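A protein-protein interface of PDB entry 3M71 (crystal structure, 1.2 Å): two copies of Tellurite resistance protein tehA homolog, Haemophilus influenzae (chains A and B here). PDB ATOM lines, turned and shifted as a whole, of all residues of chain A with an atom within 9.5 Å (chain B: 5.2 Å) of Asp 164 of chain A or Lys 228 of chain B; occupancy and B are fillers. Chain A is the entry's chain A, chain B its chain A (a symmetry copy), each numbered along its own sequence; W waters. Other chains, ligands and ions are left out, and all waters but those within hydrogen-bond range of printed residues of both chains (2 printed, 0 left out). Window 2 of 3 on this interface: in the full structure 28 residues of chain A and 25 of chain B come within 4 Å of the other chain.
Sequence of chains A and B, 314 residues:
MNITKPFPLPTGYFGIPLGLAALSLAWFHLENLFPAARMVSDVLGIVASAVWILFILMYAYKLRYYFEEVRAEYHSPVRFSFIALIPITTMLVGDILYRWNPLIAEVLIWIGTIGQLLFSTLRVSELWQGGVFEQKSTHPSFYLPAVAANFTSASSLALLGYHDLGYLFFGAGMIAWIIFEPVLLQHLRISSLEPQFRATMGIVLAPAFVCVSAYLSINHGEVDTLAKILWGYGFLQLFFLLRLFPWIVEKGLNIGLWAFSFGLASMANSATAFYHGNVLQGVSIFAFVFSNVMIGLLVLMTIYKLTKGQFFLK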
ATOM      1  N   SER A 153      21.071  15.521 -20.693  1.00  0.00           N
ATOM      2  CA  SER A 153      20.620  16.573 -19.783  1.00  0.00           C
ATOM      3  C   SER A 153      21.799  17.368 -19.231  1.00  0.00           C
ATOM      4  O   SER A 153      21.713  18.602 -19.138  1.00  0.00           O
ATOM      5  CB  SER A 153      19.792  16.005 -18.644  1.00  0.00           C
ATOM      6  OG  SER A 153      18.508  15.582 -19.073  1.00  0.00           O
ATOM      7  N   ALA A 154      22.872  16.691 -18.830  1.00  0.00           N
ATOM      8  CA  ALA A 154      24.019  17.378 -18.286  1.00  0.00           C
ATOM      9  C   ALA A 154      24.558  18.433 -19.232  1.00  0.00           C
ATOM     10  O   ALA A 154      24.799  19.578 -18.848  1.00  0.00           O
ATOM     11  CB  ALA A 154      25.081  16.382 -17.908  1.00  0.00           C
ATOM     12  N   LEU A 157      21.931  21.305 -19.950  1.00  0.00           N
ATOM     13  CA  LEU A 157      21.790  22.222 -18.831  1.00  0.00           C
ATOM     14  C   LEU A 157      23.039  23.115 -18.742  1.00  0.00           C
ATOM     15  O   LEU A 157      22.907  24.312 -18.424  1.00  0.00           O
ATOM     16  CB  LEU A 157      21.558  21.432 -17.527  1.00  0.00           C
ATOM     17  CG  LEU A 157      20.161  20.852 -17.424  1.00  0.00           C
ATOM     18  CD1 LEU A 157      20.054  19.932 -16.234  1.00  0.00           C
ATOM     19  CD2 LEU A 157      19.085  21.838 -17.319  1.00  0.00           C
ATOM     20  N   ALA A 158      24.227  22.582 -18.986  1.00  0.00           N
ATOM     21  CA  ALA A 158      25.431  23.392 -19.038  1.00  0.00           C
ATOM     22  C   ALA A 158      25.325  24.477 -20.108  1.00  0.00           C
ATOM     23  O   ALA A 158      25.724  25.634 -19.875  1.00  0.00           O
ATOM     24  CB  ALA A 158      26.671  22.545 -19.279  1.00  0.00           C
ATOM     25  N   LEU A 159      24.804  24.136 -21.285  1.00  0.00           N
ATOM     26  CA  LEU A 159      24.601  25.125 -22.351  1.00  0.00           C
ATOM     27  C   LEU A 159      23.784  26.312 -21.832  1.00  0.00           C
ATOM     28  O   LEU A 159      24.052  27.470 -22.204  1.00  0.00           O
ATOM     29  CB  LEU A 159      23.938  24.457 -23.569  1.00  0.00           C
ATOM     30  CG  LEU A 159      23.624  25.367 -24.764  1.00  0.00           C
ATOM     31  CD1 LEU A 159      24.927  25.929 -25.344  1.00  0.00           C
ATOM     32  CD2 LEU A 159      22.871  24.598 -25.785  1.00  0.00           C
ATOM     33  N   LEU A 160      22.744  26.034 -21.043  1.00  0.00           N
ATOM     34  CA  LEU A 160      21.857  27.036 -20.480  1.00  0.00           C
ATOM     35  C   LEU A 160      22.451  27.762 -19.278  1.00  0.00           C
ATOM     36  O   LEU A 160      21.847  28.705 -18.756  1.00  0.00           O
ATOM     37  CB  LEU A 160      20.549  26.400 -20.036  1.00  0.00           C
ATOM     38  CG  LEU A 160      19.694  25.751 -21.094  1.00  0.00           C
ATOM     39  CD1 LEU A 160      18.427  25.215 -20.477  1.00  0.00           C
ATOM     40  CD2 LEU A 160      19.352  26.748 -22.199  1.00  0.00           C
ATOM     41  N   GLY A 161      23.639  27.378 -18.847  1.00  0.00           N
ATOM     42  CA  GLY A 161      24.294  28.008 -17.711  1.00  0.00           C
ATOM     43  C   GLY A 161      24.124  27.361 -16.361  1.00  0.00           C
ATOM     44  O   GLY A 161      24.560  27.928 -15.359  1.00  0.00           O
ATOM     45  N   TYR A 162      23.513  26.188 -16.323  1.00  0.00           N
ATOM     46  CA  TYR A 162      23.236  25.493 -15.060  1.00  0.00           C
ATOM     47  C   TYR A 162      24.281  24.411 -14.826  1.00  0.00           C
ATOM     48  O   TYR A 162      23.975  23.213 -14.852  1.00  0.00           O
ATOM     49  CB  TYR A 162      21.824  24.920 -15.023  1.00  0.00           C
ATOM     50  CG  TYR A 162      20.715  25.913 -15.198  1.00  0.00           C
ATOM     51  CD1 TYR A 162      20.281  26.686 -14.129  1.00  0.00           C
ATOM     52  CD2 TYR A 162      20.036  26.022 -16.388  1.00  0.00           C
ATOM     53  CE1 TYR A 162      19.261  27.592 -14.292  1.00  0.00           C
ATOM     54  CE2 TYR A 162      19.007  26.929 -16.569  1.00  0.00           C
ATOM     55  CZ  TYR A 162      18.649  27.718 -15.528  1.00  0.00           C
ATOM     56  OH  TYR A 162      17.619  28.637 -15.641  1.00  0.00           O
ATOM     57  N   HIS A 163      25.525  24.809 -14.626  1.00  0.00           N
ATOM     58  CA  HIS A 163      26.629  23.853 -14.600  1.00  0.00           C
ATOM     59  C   HIS A 163      26.527  22.910 -13.425  1.00  0.00           C
ATOM     60  O   HIS A 163      26.758  21.711 -13.590  1.00  0.00           O
ATOM     61  CB  HIS A 163      27.964  24.559 -14.592  1.00  0.00           C
ATOM     62  CG  HIS A 163      28.213  25.331 -15.843  1.00  0.00           C
ATOM     63  ND1 HIS A 163      27.645  26.567 -16.060  1.00  0.00           N
ATOM     64  CD2 HIS A 163      28.902  25.014 -16.968  1.00  0.00           C
ATOM     65  CE1 HIS A 163      28.025  26.997 -17.253  1.00  0.00           C
ATOM     66  NE2 HIS A 163      28.778  26.083 -17.828  1.00  0.00           N
ATOM     67  N   ASP A 164      26.212  23.397 -12.233  1.00  0.00           N
ATOM     68  CA  ASP A 164      26.157  22.511 -11.076  1.00  0.00           C
ATOM     69  C   ASP A 164      25.005  21.511 -11.154  1.00  0.00           C
ATOM     70  O   ASP A 164      25.193  20.329 -10.846  1.00  0.00           O
ATOM     71  CB  ASP A 164      26.097  23.292  -9.764  1.00  0.00           C
ATOM     72  CG  ASP A 164      27.391  23.930  -9.417  1.00  0.00           C
ATOM     73  OD1 ASP A 164      28.447  23.510  -9.953  1.00  0.00           O
ATOM     74  OD2 ASP A 164      27.365  24.873  -8.603  1.00  0.00           O
ATOM     75  N   LEU A 165      23.834  21.925 -11.629  1.00  0.00           N
ATOM     76  CA  LEU A 165      22.763  20.991 -11.902  1.00  0.00           C
ATOM     77  C   LEU A 165      23.210  19.983 -12.980  1.00  0.00           C
ATOM     78  O   LEU A 165      22.947  18.776 -12.888  1.00  0.00           O
ATOM     79  CB  LEU A 165      21.508  21.760 -12.270  1.00  0.00           C
ATOM     80  CG  LEU A 165      20.279  20.905 -12.450  1.00  0.00           C
ATOM     81  CD1 LEU A 165      19.939  20.150 -11.174  1.00  0.00           C
ATOM     82  CD2 LEU A 165      19.157  21.766 -12.932  1.00  0.00           C
ATOM     83  N   GLY A 166      23.945  20.471 -13.988  1.00  0.00           N
ATOM     84  CA  GLY A 166      24.490  19.598 -15.009  1.00  0.00           C
ATOM     85  C   GLY A 166      25.379  18.513 -14.406  1.00  0.00           C
ATOM     86  O   GLY A 166      25.334  17.363 -14.856  1.00  0.00           O
ATOM     87  N   TYR A 167      26.223  18.874 -13.452  1.00  0.00           N
ATOM     88  CA  TYR A 167      27.057  17.872 -12.792  1.00  0.00           C
ATOM     89  C   TYR A 167      26.264  16.805 -12.090  1.00  0.00           C
ATOM     90  O   TYR A 167      26.718  15.669 -12.044  1.00  0.00           O
ATOM     91  CB  TYR A 167      28.067  18.488 -11.808  1.00  0.00           C
ATOM     92  CG  TYR A 167      29.354  19.023 -12.414  1.00  0.00           C
ATOM     93  CD1 TYR A 167      29.673  20.348 -12.414  1.00  0.00           C
ATOM     94  CD2 TYR A 167      30.236  18.187 -13.042  1.00  0.00           C
ATOM     95  CE1 TYR A 167      30.867  20.819 -12.963  1.00  0.00           C
ATOM     96  CE2 TYR A 167      31.439  18.654 -13.544  1.00  0.00           C
ATOM     97  CZ  TYR A 167      31.740  19.966 -13.503  1.00  0.00           C
ATOM     98  OH  TYR A 167      32.936  20.460 -14.061  1.00  0.00           O
ATOM     99  N   LEU A 168      25.092  17.138 -11.542  1.00  0.00           N
ATOM    100  CA  LEU A 168      24.264  16.102 -10.903  1.00  0.00           C
ATOM    101  C   LEU A 168      23.820  15.082 -11.948  1.00  0.00           C
ATOM    102  O   LEU A 168      23.941  13.879 -11.743  1.00  0.00           O
ATOM    103  CB  LEU A 168      23.024  16.678 -10.209  1.00  0.00           C
ATOM    104  CG  LEU A 168      23.162  17.686  -9.118  1.00  0.00           C
ATOM    105  CD1 LEU A 168      21.895  18.070  -8.474  1.00  0.00           C
ATOM    106  CD2 LEU A 168      23.927  17.054  -8.111  1.00  0.00           C
ATOM    107  N   PHE A 169      23.286  15.571 -13.078  1.00  0.00           N
ATOM    108  CA  PHE A 169      22.899  14.654 -14.151  1.00  0.00           C
ATOM    109  C   PHE A 169      24.106  13.861 -14.691  1.00  0.00           C
ATOM    110  O   PHE A 169      23.991  12.680 -15.012  1.00  0.00           O
ATOM    111  CB  PHE A 169      22.184  15.393 -15.284  1.00  0.00           C
ATOM    112  CG  PHE A 169      20.739  15.739 -14.944  1.00  0.00           C
ATOM    113  CD1 PHE A 169      19.718  14.825 -15.145  1.00  0.00           C
ATOM    114  CD2 PHE A 169      20.405  16.943 -14.368  1.00  0.00           C
ATOM    115  CE1 PHE A 169      18.429  15.083 -14.825  1.00  0.00           C
ATOM    116  CE2 PHE A 169      19.069  17.215 -14.030  1.00  0.00           C
ATOM    117  CZ  PHE A 169      18.106  16.297 -14.252  1.00  0.00           C
ATOM    118  N   PHE A 170      25.259  14.536 -14.811  1.00  0.00           N
ATOM    119  CA  PHE A 170      26.450  13.889 -15.286  1.00  0.00           C
ATOM    120  C   PHE A 170      26.835  12.717 -14.361  1.00  0.00           C
ATOM    121  O   PHE A 170      27.159  11.616 -14.846  1.00  0.00           O
ATOM    122  CB  PHE A 170      27.607  14.901 -15.348  1.00  0.00           C
ATOM    123  CG  PHE A 170      28.895  14.290 -15.763  1.00  0.00           C
ATOM    124  CD1 PHE A 170      29.125  13.962 -17.074  1.00  0.00           C
ATOM    125  CD2 PHE A 170      29.845  13.931 -14.834  1.00  0.00           C
ATOM    126  CE1 PHE A 170      30.278  13.294 -17.447  1.00  0.00           C
ATOM    127  CE2 PHE A 170      31.005  13.287 -15.220  1.00  0.00           C
ATOM    128  CZ  PHE A 170      31.208  12.962 -16.537  1.00  0.00           C
ATOM    129  N   GLY A 171      26.832  12.956 -13.070  1.00  0.00           N
ATOM    130  CA  GLY A 171      27.169  11.919 -12.139  1.00  0.00           C
ATOM    131  C   GLY A 171      26.190  10.760 -12.139  1.00  0.00           C
ATOM    132  O   GLY A 171      26.602   9.585 -12.027  1.00  0.00           O
ATOM    133  N   ALA A 172      24.916  11.059 -12.265  1.00  0.00           N
ATOM    134  CA  ALA A 172      23.908  10.024 -12.372  1.00  0.00           C
ATOM    135  C   ALA A 172      24.226   9.135 -13.575  1.00  0.00           C
ATOM    136  O   ALA A 172      24.201   7.909 -13.491  1.00  0.00           O
ATOM    137  CB  ALA A 172      22.518  10.632 -12.471  1.00  0.00           C
ATOM    138  N   GLY A 173      24.515   9.752 -14.729  1.00  0.00           N
ATOM    139  CA  GLY A 173      24.851   8.966 -15.908  1.00  0.00           C
ATOM    140  C   GLY A 173      26.137   8.169 -15.802  1.00  0.00           C
ATOM    141  O   GLY A 173      26.216   7.025 -16.258  1.00  0.00           O
ATOM    142  N   ILE A 175      27.928   7.118 -13.090  1.00  0.00           N
ATOM    143  CA  ILE A 175      27.879   6.017 -12.170  1.00  0.00           C
ATOM    144  C   ILE A 175      26.888   4.955 -12.671  1.00  0.00           C
ATOM    145  O   ILE A 175      27.201   3.754 -12.580  1.00  0.00           O
ATOM    146  CB  ILE A 175      27.678   6.488 -10.723  1.00  0.00           C
ATOM    147  CG1 ILE A 175      28.857   7.361 -10.282  1.00  0.00           C
ATOM    148  CG2 ILE A 175      27.492   5.315  -9.782  1.00  0.00           C
ATOM    149  CD1 ILE A 175      28.700   8.042  -8.942  1.00  0.00           C
ATOM    150  N   TYR A 215      31.009  15.847 -20.098  1.00  0.00           N
ATOM    151  CA  TYR A 215      31.956  16.360 -19.141  1.00  0.00           C
ATOM    152  C   TYR A 215      32.633  17.651 -19.611  1.00  0.00           C
ATOM    153  O   TYR A 215      32.711  18.645 -18.904  1.00  0.00           O
ATOM    154  CB  TYR A 215      33.010  15.300 -18.811  1.00  0.00           C
ATOM    155  CG  TYR A 215      33.997  15.747 -17.820  1.00  0.00           C
ATOM    156  CD1 TYR A 215      33.625  16.070 -16.527  1.00  0.00           C
ATOM    157  CD2 TYR A 215      35.335  15.868 -18.154  1.00  0.00           C
ATOM    158  CE1 TYR A 215      34.539  16.486 -15.592  1.00  0.00           C
ATOM    159  CE2 TYR A 215      36.297  16.290 -17.201  1.00  0.00           C
ATOM    160  CZ  TYR A 215      35.855  16.617 -15.911  1.00  0.00           C
ATOM    161  OH  TYR A 215      36.738  17.044 -14.962  1.00  0.00           O
ATOM    162  N   SER A 217      31.562  19.654 -21.906  1.00  0.00           N
ATOM    163  CA  SER A 217      30.615  20.731 -22.074  1.00  0.00           C
ATOM    164  C   SER A 217      30.339  21.455 -20.772  1.00  0.00           C
ATOM    165  O   SER A 217      30.032  22.664 -20.820  1.00  0.00           O
ATOM    166  CB  SER A 217      29.272  20.271 -22.651  1.00  0.00           C
ATOM    167  OG  SER A 217      29.432  19.676 -23.906  1.00  0.00           O
ATOM    168  N   ILE A 218      30.458  20.758 -19.634  1.00  0.00           N
ATOM    169  CA  ILE A 218      30.219  21.353 -18.313  1.00  0.00           C
ATOM    170  C   ILE A 218      31.433  22.033 -17.775  1.00  0.00           C
ATOM    171  O   ILE A 218      31.373  23.114 -17.189  1.00  0.00           O
ATOM    172  CB  ILE A 218      29.812  20.300 -17.286  1.00  0.00           C
ATOM    173  CG1 ILE A 218      28.594  19.526 -17.733  1.00  0.00           C
ATOM    174  CG2 ILE A 218      29.572  20.928 -15.935  1.00  0.00           C
ATOM    175  CD1 ILE A 218      28.467  18.183 -17.023  1.00  0.00           C
ATOM    176  N   ASN A 219      32.557  21.383 -17.965  1.00  0.00           N
ATOM    177  CA  ASN A 219      33.802  21.836 -17.367  1.00  0.00           C
ATOM    178  C   ASN A 219      34.495  22.869 -18.203  1.00  0.00           C
ATOM    179  O   ASN A 219      35.691  23.147 -17.991  1.00  0.00           O
ATOM    180  CB  ASN A 219      34.680  20.681 -16.966  1.00  0.00           C
ATOM    181  CG  ASN A 219      35.588  20.274 -18.024  1.00  0.00           C
ATOM    182  OD1 ASN A 219      35.374  20.618 -19.199  1.00  0.00           O
ATOM    183  ND2 ASN A 219      36.694  19.599 -17.650  1.00  0.00           N
ATOM    184  N   HIS A 220      33.770  23.486 -19.131  1.00  0.00           N
ATOM    185  CA  HIS A 220      34.296  24.588 -19.938  1.00  0.00           C
ATOM    186  C   HIS A 220      35.429  24.156 -20.901  1.00  0.00           C
ATOM    187  O   HIS A 220      36.331  24.946 -21.291  1.00  0.00           O
ATOM    188  CB  HIS A 220      34.731  25.787 -19.041  1.00  0.00           C
ATOM    189  CG  HIS A 220      33.684  26.224 -18.036  1.00  0.00           C
ATOM    190  ND1 HIS A 220      32.613  27.029 -18.371  1.00  0.00           N
ATOM    191  CD2 HIS A 220      33.553  25.965 -16.714  1.00  0.00           C
ATOM    192  CE1 HIS A 220      31.874  27.249 -17.298  1.00  0.00           C
ATOM    193  NE2 HIS A 220      32.411  26.600 -16.282  1.00  0.00           N
ATOM    194  N   VAL B 223      33.527  21.289  -1.821  1.00  0.00           N
ATOM    195  CA  VAL B 223      32.514  20.727  -2.694  1.00  0.00           C
ATOM    196  C   VAL B 223      32.964  20.792  -4.135  1.00  0.00           C
ATOM    197  O   VAL B 223      32.779  21.800  -4.853  1.00  0.00           O
ATOM    198  CB  VAL B 223      31.171  21.417  -2.503  1.00  0.00           C
ATOM    199  CG1 VAL B 223      30.100  20.780  -3.402  1.00  0.00           C
ATOM    200  CG2 VAL B 223      30.747  21.349  -1.055  1.00  0.00           C
ATOM    201  N   ASP B 224      33.558  19.740  -4.622  1.00  0.00           N
ATOM    202  CA  ASP B 224      34.226  19.679  -5.891  1.00  0.00           C
ATOM    203  C   ASP B 224      33.470  18.816  -6.869  1.00  0.00           C
ATOM    204  O   ASP B 224      32.315  18.436  -6.671  1.00  0.00           O
ATOM    205  CB  ASP B 224      35.659  19.193  -5.653  1.00  0.00           C
ATOM    206  CG  ASP B 224      35.736  17.799  -5.108  1.00  0.00           C
ATOM    207  OD1 ASP B 224      34.700  17.148  -4.974  1.00  0.00           O
ATOM    208  OD2 ASP B 224      36.904  17.325  -4.861  1.00  0.00           O
ATOM    209  N   THR B 225      34.096  18.511  -7.995  1.00  0.00           N
ATOM    210  CA  THR B 225      33.439  17.738  -9.056  1.00  0.00           C
ATOM    211  C   THR B 225      33.022  16.355  -8.567  1.00  0.00           C
ATOM    212  O   THR B 225      31.878  15.932  -8.816  1.00  0.00           O
ATOM    213  CB  THR B 225      34.314  17.640 -10.294  1.00  0.00           C
ATOM    214  OG1 THR B 225      34.420  18.966 -10.802  1.00  0.00           O
ATOM    215  CG2 THR B 225      33.746  16.686 -11.311  1.00  0.00           C
ATOM    216  N   LEU B 226      33.906  15.636  -7.854  1.00  0.00           N
ATOM    217  CA  LEU B 226      33.545  14.353  -7.301  1.00  0.00           C
ATOM    218  C   LEU B 226      32.341  14.443  -6.403  1.00  0.00           C
ATOM    219  O   LEU B 226      31.418  13.624  -6.494  1.00  0.00           O
ATOM    220  CB  LEU B 226      34.707  13.705  -6.572  1.00  0.00           C
ATOM    221  CG  LEU B 226      34.390  12.371  -5.906  1.00  0.00           C
ATOM    222  CD1 LEU B 226      33.870  11.328  -6.892  1.00  0.00           C
ATOM    223  CD2 LEU B 226      35.589  11.838  -5.136  1.00  0.00           C
ATOM    224  N   ALA B 227      32.290  15.427  -5.504  1.00  0.00           N
ATOM    225  CA  ALA B 227      31.161  15.552  -4.598  1.00  0.00           C
ATOM    226  C   ALA B 227      29.846  15.735  -5.368  1.00  0.00           C
ATOM    227  O   ALA B 227      28.832  15.156  -5.029  1.00  0.00           O
ATOM    228  CB  ALA B 227      31.391  16.698  -3.618  1.00  0.00           C
ATOM    229  N   LYS B 228      29.855  16.600  -6.388  1.00  0.00           N
ATOM    230  CA  LYS B 228      28.656  16.856  -7.165  1.00  0.00           C
ATOM    231  C   LYS B 228      28.220  15.588  -7.947  1.00  0.00           C
ATOM    232  O   LYS B 228      27.017  15.297  -8.023  1.00  0.00           O
ATOM    233  CB  LYS B 228      28.893  18.006  -8.137  1.00  0.00           C
ATOM    234  CG  LYS B 228      29.135  19.336  -7.465  1.00  0.00           C
ATOM    235  CD  LYS B 228      29.624  20.430  -8.450  1.00  0.00           C
ATOM    236  CE  LYS B 228      30.277  21.598  -7.771  1.00  0.00           C
ATOM    237  NZ  LYS B 228      30.799  22.545  -8.812  1.00  0.00           N
ATOM    238  N   ILE B 229      29.183  14.855  -8.480  1.00  0.00           N
ATOM    239  CA  ILE B 229      28.905  13.589  -9.159  1.00  0.00           C
ATOM    240  C   ILE B 229      28.209  12.595  -8.254  1.00  0.00           C
ATOM    241  O   ILE B 229      27.199  11.963  -8.621  1.00  0.00           O
ATOM    242  CB  ILE B 229      30.220  13.021  -9.721  1.00  0.00           C
ATOM    243  CG1 ILE B 229      30.593  13.755 -11.006  1.00  0.00           C
ATOM    244  CG2 ILE B 229      30.160  11.481  -9.943  1.00  0.00           C
ATOM    245  CD1 ILE B 229      31.954  13.426 -11.576  1.00  0.00           C
ATOM    246  N   LEU B 230      28.718  12.457  -7.038  1.00  0.00           N
ATOM    247  CA  LEU B 230      28.132  11.531  -6.065  1.00  0.00           C
ATOM    248  C   LEU B 230      26.721  11.955  -5.686  1.00  0.00           C
ATOM    249  O   LEU B 230      25.820  11.118  -5.574  1.00  0.00           O
ATOM    250  CB  LEU B 230      29.028  11.446  -4.832  1.00  0.00           C
ATOM    251  CG  LEU B 230      30.390  10.793  -5.025  1.00  0.00           C
ATOM    252  CD1 LEU B 230      31.290  11.059  -3.874  1.00  0.00           C
ATOM    253  CD2 LEU B 230      30.241   9.296  -5.269  1.00  0.00           C
ATOM    254  N   TRP B 231      26.508  13.264  -5.459  1.00  0.00           N
ATOM    255  CA  TRP B 231      25.173  13.731  -5.145  1.00  0.00           C
ATOM    256  C   TRP B 231      24.203  13.415  -6.264  1.00  0.00           C
ATOM    257  O   TRP B 231      23.059  13.054  -6.000  1.00  0.00           O
ATOM    258  CB  TRP B 231      25.153  15.267  -4.841  1.00  0.00           C
ATOM    259  CG  TRP B 231      24.771  15.607  -3.478  1.00  0.00           C
ATOM    260  CD1 TRP B 231      24.906  14.865  -2.363  1.00  0.00           C
ATOM    261  CD2 TRP B 231      24.154  16.815  -3.090  1.00  0.00           C
ATOM    262  NE1 TRP B 231      24.379  15.529  -1.282  1.00  0.00           N
ATOM    263  CE2 TRP B 231      23.881  16.722  -1.721  1.00  0.00           C
ATOM    264  CE3 TRP B 231      23.738  17.945  -3.785  1.00  0.00           C
ATOM    265  CZ2 TRP B 231      23.241  17.755  -0.997  1.00  0.00           C
ATOM    266  CZ3 TRP B 231      23.138  18.981  -3.078  1.00  0.00           C
ATOM    267  CH2 TRP B 231      22.862  18.833  -1.712  1.00  0.00           C
ATOM    268  N   GLY B 232      24.614  13.560  -7.522  1.00  0.00           N
ATOM    269  CA  GLY B 232      23.711  13.302  -8.582  1.00  0.00           C
ATOM    270  C   GLY B 232      23.215  11.856  -8.634  1.00  0.00           C
ATOM    271  O   GLY B 232      22.029  11.599  -8.787  1.00  0.00           O
ATOM    272  N   PHE B 274      27.270  21.183   1.216  1.00  0.00           N
ATOM    273  CA  PHE B 274      26.901  21.866  -0.022  1.00  0.00           C
ATOM    274  C   PHE B 274      26.465  23.304   0.306  1.00  0.00           C
ATOM    275  O   PHE B 274      26.822  24.259  -0.376  1.00  0.00           O
ATOM    276  CB  PHE B 274      25.827  21.095  -0.800  1.00  0.00           C
ATOM    277  CG  PHE B 274      26.408  19.996  -1.704  1.00  0.00           C
ATOM    278  CD1 PHE B 274      26.899  18.832  -1.191  1.00  0.00           C
ATOM    279  CD2 PHE B 274      26.458  20.168  -3.051  1.00  0.00           C
ATOM    280  CE1 PHE B 274      27.454  17.845  -1.988  1.00  0.00           C
ATOM    281  CE2 PHE B 274      26.974  19.189  -3.856  1.00  0.00           C
ATOM    282  CZ  PHE B 274      27.472  18.017  -3.317  1.00  0.00           C
ATOM    283  N   VAL B 279      26.888  25.731  -2.977  1.00  0.00           N
ATOM    284  CA  VAL B 279      26.580  24.913  -4.152  1.00  0.00           C
ATOM    285  C   VAL B 279      25.193  24.352  -3.990  1.00  0.00           C
ATOM    286  O   VAL B 279      24.875  23.683  -3.015  1.00  0.00           O
ATOM    287  CB  VAL B 279      27.615  23.740  -4.305  1.00  0.00           C
ATOM    288  CG1 VAL B 279      27.245  22.854  -5.466  1.00  0.00           C
ATOM    289  CG2 VAL B 279      29.027  24.305  -4.475  1.00  0.00           C
ATOM    290  N   LEU B 280      24.325  24.659  -4.926  1.00  0.00           N
ATOM    291  CA  LEU B 280      22.962  24.125  -4.950  1.00  0.00           C
ATOM    292  C   LEU B 280      22.295  24.291  -3.590  1.00  0.00           C
ATOM    293  O   LEU B 280      21.740  23.355  -3.007  1.00  0.00           O
ATOM    294  CB  LEU B 280      22.974  22.662  -5.407  1.00  0.00           C
ATOM    295  CG  LEU B 280      23.575  22.410  -6.778  1.00  0.00           C
ATOM    296  CD1 LEU B 280      23.898  20.890  -6.944  1.00  0.00           C
ATOM    297  CD2 LEU B 280      22.583  22.875  -7.825  1.00  0.00           C
HETATM  298  O   HOH W   1      35.406  19.127 -13.353  1.00  0.00           O
HETATM  299  O   HOH W   2      25.195  26.019  -7.399  1.00  0.00           O
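The side-chain carboxylate (OD1) of Asp 164 of chain A lies within salt-bridge range of the side-chain amino group (NZ) of Lys 228 of chain B, 2.8 Å away.
The backbone carbonyl oxygen (O) of Phe 274 of chain B is in hydrogen-bond range of the backbone NH (N) of Val 279 of chain B, at 3.0 Å.
OD2 of Asp 164 of chain A touches CG1 of Val 279 of chain B, 3.7 Å away.
Thr 225 of chain B touches Tyr 167 of chain A (CG2 to CE2, 3.8 Å).
CB of Tyr 167 of chain A touches CB of Lys 228 of chain B, at 3.8 Å.
CD2 of Leu 168 of chain A touches O of Lys 228 of chain B, 3.6 Å away.
CB of Trp 231 of chain B touches CD2 of Leu 168 of chain A, 3.9 Å away.
Gly 232 of chain B touches Leu 168 of chain A.
Leu 280 of chain B touches Leu 168 of chain A.
Phe 170 of chain A touches Ile 229 of chain B.
Gly 232 of chain B touches Ala 172 of chain A.
CG2 of Ile 229 of chain B touches CD1 of Ile 175 of chain A (3.9 Å).
Printed residues of chain B within 4 Å of Asp 164 of chain A: Lys 228 (2.8 Å) and Val 279 (3.7 Å).
Of chain A, only Asp 164 (2.8 Å), Tyr 167 (3.8 Å) and Leu 168 (3.6 Å) come within 4 Å of Lys 228 of chain B.
Of the printed residues of chain B, Tyr 167 of chain A touches Thr 225 (3.8 Å) and Lys 228 (3.8 Å).
Of the printed residues of chain A, Ile 229 of chain B touches Phe 170 (3.8 Å), Gly 171 (3.5 Å) and Ile 175 (3.9 Å).
Of the printed residues of chain B, Gly 171 of chain A touches Ile 229 (3.5 Å).
Printed residues of chain B within 4 Å of Phe 170 of chain A: Ile 229 (3.8 Å).
Of the printed residues of chain A, Leu 280 of chain B touches Leu 168 (3.8 Å).
The nearest residue of chain A that does not touch Lys 228 of chain B is Gly 171 of chain A (5.3 Å).
Of the 25 printed residues of chain A, 7 touch a printed residue of chain B.
Hydrophobic or aromatic side chains of chain A within 4 Å of the printed part of chain B: Tyr 167, Leu 168, Phe 170, Ala 172 and Ile 175.
Of the 13 printed residues of chain B, 7 touch a printed residue of chain A.
Among the printed residues, 12 pairs touch across the chains.
Among the printed residues, Asp or Glu carboxylates within 4 Å of a Lys or Arg side-chain nitrogen of the other chain: Asp 164 of chain A with Lys 228 of chain B (2.8 Å).
No position is printed for both chains.
Water W2 lies within hydrogen-bond range of OD2 of Asp 164 of chain A (2.7 Å) and N of Leu 280 of chain B (3.0 Å).
Water W1 lies within hydrogen-bond range of OG1 of Thr 225 of chain B (2.7 Å), OH of Tyr 167 of chain A (2.9 Å) and OH of Tyr 215 of chain A (2.9 Å).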
